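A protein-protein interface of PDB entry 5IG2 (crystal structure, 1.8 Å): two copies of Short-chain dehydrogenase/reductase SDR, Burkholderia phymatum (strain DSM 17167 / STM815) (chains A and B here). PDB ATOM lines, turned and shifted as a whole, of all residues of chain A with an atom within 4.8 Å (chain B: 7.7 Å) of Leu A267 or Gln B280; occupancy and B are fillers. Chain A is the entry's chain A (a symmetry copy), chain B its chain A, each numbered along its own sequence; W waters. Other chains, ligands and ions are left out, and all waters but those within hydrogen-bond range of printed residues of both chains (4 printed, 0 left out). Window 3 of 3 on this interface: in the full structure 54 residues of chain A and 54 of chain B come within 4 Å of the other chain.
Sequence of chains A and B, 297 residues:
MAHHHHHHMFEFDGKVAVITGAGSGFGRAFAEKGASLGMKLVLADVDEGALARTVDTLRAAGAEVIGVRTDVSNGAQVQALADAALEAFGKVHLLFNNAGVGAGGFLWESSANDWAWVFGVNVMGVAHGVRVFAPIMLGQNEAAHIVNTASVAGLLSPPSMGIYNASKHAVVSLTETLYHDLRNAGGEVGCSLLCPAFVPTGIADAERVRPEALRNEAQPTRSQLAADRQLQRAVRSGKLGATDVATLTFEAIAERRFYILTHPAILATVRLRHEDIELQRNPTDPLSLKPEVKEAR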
ATOM      1  N   ARG A 257      25.183  39.595  -7.733  1.00  0.00           N
ATOM      2  CA  ARG A 257      25.834  38.297  -7.781  1.00  0.00           C
ATOM      3  C   ARG A 257      24.789  37.211  -8.009  1.00  0.00           C
ATOM      4  O   ARG A 257      23.734  37.208  -7.362  1.00  0.00           O
ATOM      5  CB  ARG A 257      26.601  38.039  -6.487  1.00  0.00           C
ATOM      6  CG  ARG A 257      27.107  36.614  -6.386  1.00  0.00           C
ATOM      7  CD  ARG A 257      28.132  36.421  -5.283  1.00  0.00           C
ATOM      8  NE  ARG A 257      27.616  36.773  -3.972  1.00  0.00           N
ATOM      9  CZ  ARG A 257      27.879  37.924  -3.369  1.00  0.00           C
ATOM     10  NH1 ARG A 257      28.662  38.824  -3.963  1.00  0.00           N
ATOM     11  NH2 ARG A 257      27.359  38.173  -2.175  1.00  0.00           N
ATOM     12  N   TYR A 259      25.010  33.490  -7.930  1.00  0.00           N
ATOM     13  CA  TYR A 259      24.953  32.379  -6.983  1.00  0.00           C
ATOM     14  C   TYR A 259      25.055  32.882  -5.545  1.00  0.00           C
ATOM     15  O   TYR A 259      26.079  33.458  -5.154  1.00  0.00           O
ATOM     16  CB  TYR A 259      26.079  31.389  -7.260  1.00  0.00           C
ATOM     17  CG  TYR A 259      25.907  30.591  -8.539  1.00  0.00           C
ATOM     18  CD1 TYR A 259      24.906  29.626  -8.649  1.00  0.00           C
ATOM     19  CD2 TYR A 259      26.761  30.786  -9.623  1.00  0.00           C
ATOM     20  CE1 TYR A 259      24.751  28.883  -9.807  1.00  0.00           C
ATOM     21  CE2 TYR A 259      26.613  30.043 -10.800  1.00  0.00           C
ATOM     22  CZ  TYR A 259      25.607  29.092 -10.881  1.00  0.00           C
ATOM     23  OH  TYR A 259      25.445  28.348 -12.039  1.00  0.00           O
ATOM     24  N   LEU A 261      25.247  31.336  -2.114  1.00  0.00           N
ATOM     25  CA  LEU A 261      25.446  30.181  -1.244  1.00  0.00           C
ATOM     26  C   LEU A 261      25.630  30.706   0.175  1.00  0.00           C
ATOM     27  O   LEU A 261      26.720  31.143   0.552  1.00  0.00           O
ATOM     28  CB  LEU A 261      26.649  29.354  -1.683  1.00  0.00           C
ATOM     29  CG  LEU A 261      26.747  28.871  -3.132  1.00  0.00           C
ATOM     30  CD1 LEU A 261      27.760  27.741  -3.219  1.00  0.00           C
ATOM     31  CD2 LEU A 261      25.418  28.434  -3.686  1.00  0.00           C
ATOM     32  N   PRO A 264      28.500  28.165   2.461  1.00  0.00           N
ATOM     33  CA  PRO A 264      29.494  27.689   1.482  1.00  0.00           C
ATOM     34  C   PRO A 264      30.241  26.452   1.934  1.00  0.00           C
ATOM     35  O   PRO A 264      30.945  25.849   1.115  1.00  0.00           O
ATOM     36  CB  PRO A 264      30.437  28.890   1.314  1.00  0.00           C
ATOM     37  CG  PRO A 264      30.273  29.687   2.579  1.00  0.00           C
ATOM     38  CD  PRO A 264      28.843  29.487   3.017  1.00  0.00           C
ATOM     39  N   ALA A 265      30.091  26.040   3.195  1.00  0.00           N
ATOM     40  CA  ALA A 265      30.682  24.784   3.644  1.00  0.00           C
ATOM     41  C   ALA A 265      30.180  23.600   2.842  1.00  0.00           C
ATOM     42  O   ALA A 265      30.849  22.564   2.796  1.00  0.00           O
ATOM     43  CB  ALA A 265      30.373  24.554   5.122  1.00  0.00           C
ATOM     44  N   ILE A 266      29.011  23.730   2.211  1.00  0.00           N
ATOM     45  CA  ILE A 266      28.452  22.650   1.411  1.00  0.00           C
ATOM     46  C   ILE A 266      29.285  22.342   0.171  1.00  0.00           C
ATOM     47  O   ILE A 266      29.104  21.288  -0.448  1.00  0.00           O
ATOM     48  CB  ILE A 266      26.997  23.032   1.059  1.00  0.00           C
ATOM     49  CG1 ILE A 266      26.158  21.780   0.789  1.00  0.00           C
ATOM     50  CG2 ILE A 266      26.954  24.004  -0.121  1.00  0.00           C
ATOM     51  CD1 ILE A 266      26.111  20.804   1.966  1.00  0.00           C
ATOM     52  N   LEU A 267      30.222  23.216  -0.196  1.00  0.00           N
ATOM     53  CA  LEU A 267      30.833  23.108  -1.516  1.00  0.00           C
ATOM     54  C   LEU A 267      31.660  21.836  -1.669  1.00  0.00           C
ATOM     55  O   LEU A 267      31.815  21.337  -2.788  1.00  0.00           O
ATOM     56  CB  LEU A 267      31.673  24.352  -1.800  1.00  0.00           C
ATOM     57  CG  LEU A 267      30.827  25.553  -2.251  1.00  0.00           C
ATOM     58  CD1 LEU A 267      31.565  26.875  -2.056  1.00  0.00           C
ATOM     59  CD2 LEU A 267      30.398  25.371  -3.699  1.00  0.00           C
ATOM     60  N   ALA A 268      32.187  21.288  -0.570  1.00  0.00           N
ATOM     61  CA  ALA A 268      32.889  20.011  -0.668  1.00  0.00           C
ATOM     62  C   ALA A 268      31.958  18.920  -1.175  1.00  0.00           C
ATOM     63  O   ALA A 268      32.335  18.128  -2.045  1.00  0.00           O
ATOM     64  CB  ALA A 268      33.482  19.616   0.682  1.00  0.00           C
ATOM     65  N   THR A 269      30.728  18.878  -0.652  1.00  0.00           N
ATOM     66  CA  THR A 269      29.752  17.883  -1.089  1.00  0.00           C
ATOM     67  C   THR A 269      29.305  18.144  -2.524  1.00  0.00           C
ATOM     68  O   THR A 269      29.096  17.202  -3.302  1.00  0.00           O
ATOM     69  CB  THR A 269      28.548  17.884  -0.134  1.00  0.00           C
ATOM     70  OG1 THR A 269      29.013  17.735   1.214  1.00  0.00           O
ATOM     71  CG2 THR A 269      27.595  16.742  -0.450  1.00  0.00           C
ATOM     72  N   VAL A 270      29.154  19.415  -2.892  1.00  0.00           N
ATOM     73  CA  VAL A 270      28.783  19.750  -4.263  1.00  0.00           C
ATOM     74  C   VAL A 270      29.873  19.295  -5.227  1.00  0.00           C
ATOM     75  O   VAL A 270      29.597  18.677  -6.260  1.00  0.00           O
ATOM     76  CB  VAL A 270      28.496  21.259  -4.383  1.00  0.00           C
ATOM     77  CG1 VAL A 270      28.297  21.663  -5.837  1.00  0.00           C
ATOM     78  CG2 VAL A 270      27.260  21.613  -3.569  1.00  0.00           C
ATOM     79  N   ARG A 271      31.132  19.575  -4.885  1.00  0.00           N
ATOM     80  CA  ARG A 271      32.249  19.138  -5.713  1.00  0.00           C
ATOM     81  C   ARG A 271      32.235  17.627  -5.903  1.00  0.00           C
ATOM     82  O   ARG A 271      32.574  17.124  -6.982  1.00  0.00           O
ATOM     83  CB  ARG A 271      33.568  19.600  -5.080  1.00  0.00           C
ATOM     84  CG  ARG A 271      34.817  19.176  -5.835  1.00  0.00           C
ATOM     85  CD  ARG A 271      34.757  19.651  -7.278  1.00  0.00           C
ATOM     86  NE  ARG A 271      35.622  18.868  -8.155  1.00  0.00           N
ATOM     87  CZ  ARG A 271      35.371  18.657  -9.444  1.00  0.00           C
ATOM     88  NH1 ARG A 271      34.276  19.164  -9.979  1.00  0.00           N
ATOM     89  NH2 ARG A 271      36.201  17.935 -10.191  1.00  0.00           N
ATOM     90  N   HIS B 274      30.031  23.611 -13.698  1.00  0.00           N
ATOM     91  CA  HIS B 274      30.360  23.184 -12.342  1.00  0.00           C
ATOM     92  C   HIS B 274      31.351  24.143 -11.705  1.00  0.00           C
ATOM     93  O   HIS B 274      31.247  24.466 -10.514  1.00  0.00           O
ATOM     94  CB  HIS B 274      30.925  21.760 -12.361  1.00  0.00           C
ATOM     95  CG  HIS B 274      29.906  20.710 -12.669  1.00  0.00           C
ATOM     96  ND1 HIS B 274      30.242  19.391 -12.891  1.00  0.00           N
ATOM     97  CD2 HIS B 274      28.556  20.780 -12.778  1.00  0.00           C
ATOM     98  CE1 HIS B 274      29.144  18.696 -13.129  1.00  0.00           C
ATOM     99  NE2 HIS B 274      28.106  19.513 -13.066  1.00  0.00           N
ATOM    100  N   GLU B 275      32.303  24.636 -12.498  1.00  0.00           N
ATOM    101  CA  GLU B 275      33.253  25.611 -11.981  1.00  0.00           C
ATOM    102  C   GLU B 275      32.558  26.914 -11.592  1.00  0.00           C
ATOM    103  O   GLU B 275      32.885  27.505 -10.559  1.00  0.00           O
ATOM    104  CB  GLU B 275      34.351  25.865 -13.010  1.00  0.00           C
ATOM    105  CG  GLU B 275      35.513  26.654 -12.451  1.00  0.00           C
ATOM    106  CD  GLU B 275      36.549  26.978 -13.500  1.00  0.00           C
ATOM    107  OE1 GLU B 275      36.190  27.616 -14.515  1.00  0.00           O
ATOM    108  OE2 GLU B 275      37.720  26.581 -13.313  1.00  0.00           O
ATOM    109  N   ASP B 276      31.611  27.388 -12.415  1.00  0.00           N
ATOM    110  CA  ASP B 276      30.808  28.553 -12.040  1.00  0.00           C
ATOM    111  C   ASP B 276      30.239  28.387 -10.638  1.00  0.00           C
ATOM    112  O   ASP B 276      30.329  29.294  -9.802  1.00  0.00           O
ATOM    113  CB  ASP B 276      29.652  28.767 -13.024  1.00  0.00           C
ATOM    114  CG  ASP B 276      30.103  29.233 -14.405  1.00  0.00           C
ATOM    115  OD1 ASP B 276      31.285  29.617 -14.560  1.00  0.00           O
ATOM    116  OD2 ASP B 276      29.245  29.225 -15.329  1.00  0.00           O
ATOM    117  N   ILE B 277      29.643  27.221 -10.371  1.00  0.00           N
ATOM    118  CA  ILE B 277      28.973  26.984  -9.097  1.00  0.00           C
ATOM    119  C   ILE B 277      29.988  26.934  -7.965  1.00  0.00           C
ATOM    120  O   ILE B 277      29.838  27.617  -6.944  1.00  0.00           O
ATOM    121  CB  ILE B 277      28.147  25.688  -9.158  1.00  0.00           C
ATOM    122  CG1 ILE B 277      27.006  25.836 -10.171  1.00  0.00           C
ATOM    123  CG2 ILE B 277      27.630  25.317  -7.765  1.00  0.00           C
ATOM    124  CD1 ILE B 277      26.390  24.519 -10.599  1.00  0.00           C
ATOM    125  N   GLU B 278      31.030  26.116  -8.127  1.00  0.00           N
ATOM    126  CA  GLU B 278      32.039  25.981  -7.082  1.00  0.00           C
ATOM    127  C   GLU B 278      32.717  27.315  -6.761  1.00  0.00           C
ATOM    128  O   GLU B 278      33.103  27.551  -5.608  1.00  0.00           O
ATOM    129  CB  GLU B 278      33.060  24.927  -7.504  1.00  0.00           C
ATOM    130  CG  GLU B 278      32.451  23.541  -7.607  1.00  0.00           C
ATOM    131  CD  GLU B 278      33.223  22.603  -8.527  1.00  0.00           C
ATOM    132  OE1 GLU B 278      32.649  21.568  -8.939  1.00  0.00           O
ATOM    133  OE2 GLU B 278      34.399  22.899  -8.843  1.00  0.00           O
ATOM    134  N   LEU B 279      32.841  28.206  -7.750  1.00  0.00           N
ATOM    135  CA  LEU B 279      33.454  29.514  -7.559  1.00  0.00           C
ATOM    136  C   LEU B 279      32.447  30.612  -7.242  1.00  0.00           C
ATOM    137  O   LEU B 279      32.854  31.767  -7.059  1.00  0.00           O
ATOM    138  CB  LEU B 279      34.257  29.913  -8.798  1.00  0.00           C
ATOM    139  CG  LEU B 279      35.424  28.981  -9.090  1.00  0.00           C
ATOM    140  CD1 LEU B 279      36.232  29.461 -10.289  1.00  0.00           C
ATOM    141  CD2 LEU B 279      36.287  28.888  -7.856  1.00  0.00           C
ATOM    142  N   GLN B 280      31.154  30.289  -7.166  1.00  0.00           N
ATOM    143  CA  GLN B 280      30.120  31.294  -6.935  1.00  0.00           C
ATOM    144  C   GLN B 280      30.285  32.455  -7.910  1.00  0.00           C
ATOM    145  O   GLN B 280      30.206  33.630  -7.545  1.00  0.00           O
ATOM    146  CB  GLN B 280      30.143  31.760  -5.483  1.00  0.00           C
ATOM    147  CG  GLN B 280      30.115  30.586  -4.505  1.00  0.00           C
ATOM    148  CD  GLN B 280      30.491  30.984  -3.089  1.00  0.00           C
ATOM    149  OE1 GLN B 280      29.726  31.657  -2.399  1.00  0.00           O
ATOM    150  NE2 GLN B 280      31.680  30.566  -2.648  1.00  0.00           N
ATOM    151  N   ARG B 281      30.550  32.100  -9.166  1.00  0.00           N
ATOM    152  CA  ARG B 281      30.826  33.025 -10.254  1.00  0.00           C
ATOM    153  C   ARG B 281      29.607  33.096 -11.165  1.00  0.00           C
ATOM    154  O   ARG B 281      28.987  32.070 -11.453  1.00  0.00           O
ATOM    155  CB  ARG B 281      32.059  32.552 -11.036  1.00  0.00           C
ATOM    156  CG  ARG B 281      32.358  33.279 -12.347  1.00  0.00           C
ATOM    157  CD  ARG B 281      33.618  32.690 -12.994  1.00  0.00           C
ATOM    158  NE  ARG B 281      33.369  31.349 -13.524  1.00  0.00           N
ATOM    159  CZ  ARG B 281      34.316  30.492 -13.892  1.00  0.00           C
ATOM    160  NH1 ARG B 281      35.600  30.815 -13.770  1.00  0.00           N
ATOM    161  NH2 ARG B 281      33.974  29.303 -14.371  1.00  0.00           N
ATOM    162  N   ASN B 282      29.255  34.304 -11.604  1.00  0.00           N
ATOM    163  CA  ASN B 282      28.086  34.459 -12.464  1.00  0.00           C
ATOM    164  C   ASN B 282      28.215  33.565 -13.697  1.00  0.00           C
ATOM    165  O   ASN B 282      29.319  33.387 -14.220  1.00  0.00           O
ATOM    166  CB  ASN B 282      27.920  35.918 -12.876  1.00  0.00           C
ATOM    167  CG  ASN B 282      27.472  36.794 -11.714  1.00  0.00           C
ATOM    168  OD1 ASN B 282      27.244  36.306 -10.610  1.00  0.00           O
ATOM    169  ND2 ASN B 282      27.348  38.087 -11.960  1.00  0.00           N
ATOM    170  N   PRO B 283      27.119  32.979 -14.172  1.00  0.00           N
ATOM    171  CA  PRO B 283      27.208  31.953 -15.221  1.00  0.00           C
ATOM    172  C   PRO B 283      28.002  32.402 -16.439  1.00  0.00           C
ATOM    173  O   PRO B 283      27.814  33.502 -16.960  1.00  0.00           O
ATOM    174  CB  PRO B 283      25.742  31.693 -15.570  1.00  0.00           C
ATOM    175  CG  PRO B 283      25.016  31.959 -14.280  1.00  0.00           C
ATOM    176  CD  PRO B 283      25.751  33.111 -13.633  1.00  0.00           C
HETATM  177  O   HOH W   1      29.360  32.513   0.226  1.00  0.00           O
HETATM  178  O   HOH W   2      26.733  28.401 -14.693  1.00  0.00           O
HETATM  179  O   HOH W   3      27.526  34.214  -8.767  1.00  0.00           O
HETATM  180  O   HOH W   4      27.417  33.002  -2.798  1.00  0.00           O
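The guanidinium group of Arg A271 is in salt-bridge range of the side-chain carboxylate of Glu B278, 3.1 Å away.
NH2 of Arg B281 is in salt-bridge range of OE1 of Glu B275 (2.8 Å). OD1 of Asp B276 is in salt-bridge range of NH2 of Arg B281, at 2.7 Å.
Asn B282 touches Arg A257. CD2 of Tyr A259 touches O of Asp B276, 3.9 Å away. OH of Tyr A259 touches CG1 of Ile B277, 3.5 Å away. Arg B281 touches Tyr A259. OE1 of Gln B280 touches CB of Leu A261 (3.9 Å). Leu A267 touches Ile B277. CA of Glu B278 touches CD2 of Leu A267 (3.8 Å). Leu A267 touches Gln B280.
Pro A264 touches none of the printed residues of chain B. Of the printed residues of chain B, Leu A267 touches Ile B277, Glu B278 and Gln B280. Printed residues of chain B within 4 Å of Arg A271: Glu B278 (3.1 Å). Printed residues of chain A within 4 Å of Ile B277: Tyr A259 and Leu A267. Of the printed residues of chain A, Gln B280 touches Leu A261 and Leu A267. Printed residues of chain A within 4 Å of Asn B282: Arg A257. The nearest printed residue of chain B that does not touch Leu A267 is Leu B279 (5.5 Å).
Hydrophobic or aromatic side chains of chain A that line the printed part of chain B: Tyr A259, Leu A261 and Leu A267. Printed residues of chain B that touch a printed residue of chain A: Asp B276, Ile B277, Glu B278, Gln B280, Arg B281 and Asn B282. Among the printed residues, 9 pairs touch across the chains.
No position is printed for both chains. Of the 9 pairs that touch across the chains among the printed residues, none has its exchanged pair printed and touching as well.
Water W4 lies within hydrogen-bond range of the side-chain amide oxygen of Gln B280 (2.7 Å), the backbone carbonyl oxygen of Tyr A259 (2.7 Å) and the backbone NH of Leu A261 (2.8 Å). Water W2 bridges the side-chain carboxylate of Asp B276 (2.7 Å) and the side-chain hydroxyl of Tyr A259 (3.0 Å). Water W3 lies within hydrogen-bond range of the backbone NH (N) of Tyr A259 (2.7 Å), the side-chain amide oxygen (OD1) of Asn B282 (2.8 Å) and the backbone carbonyl oxygen (O) of Gln B280 (3.0 Å). Water W1 lies within hydrogen-bond range of the side-chain amide oxygen (OE1) of Gln B280 (2.8 Å) and the backbone carbonyl oxygen (O) of Leu A261 (3.0 Å).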
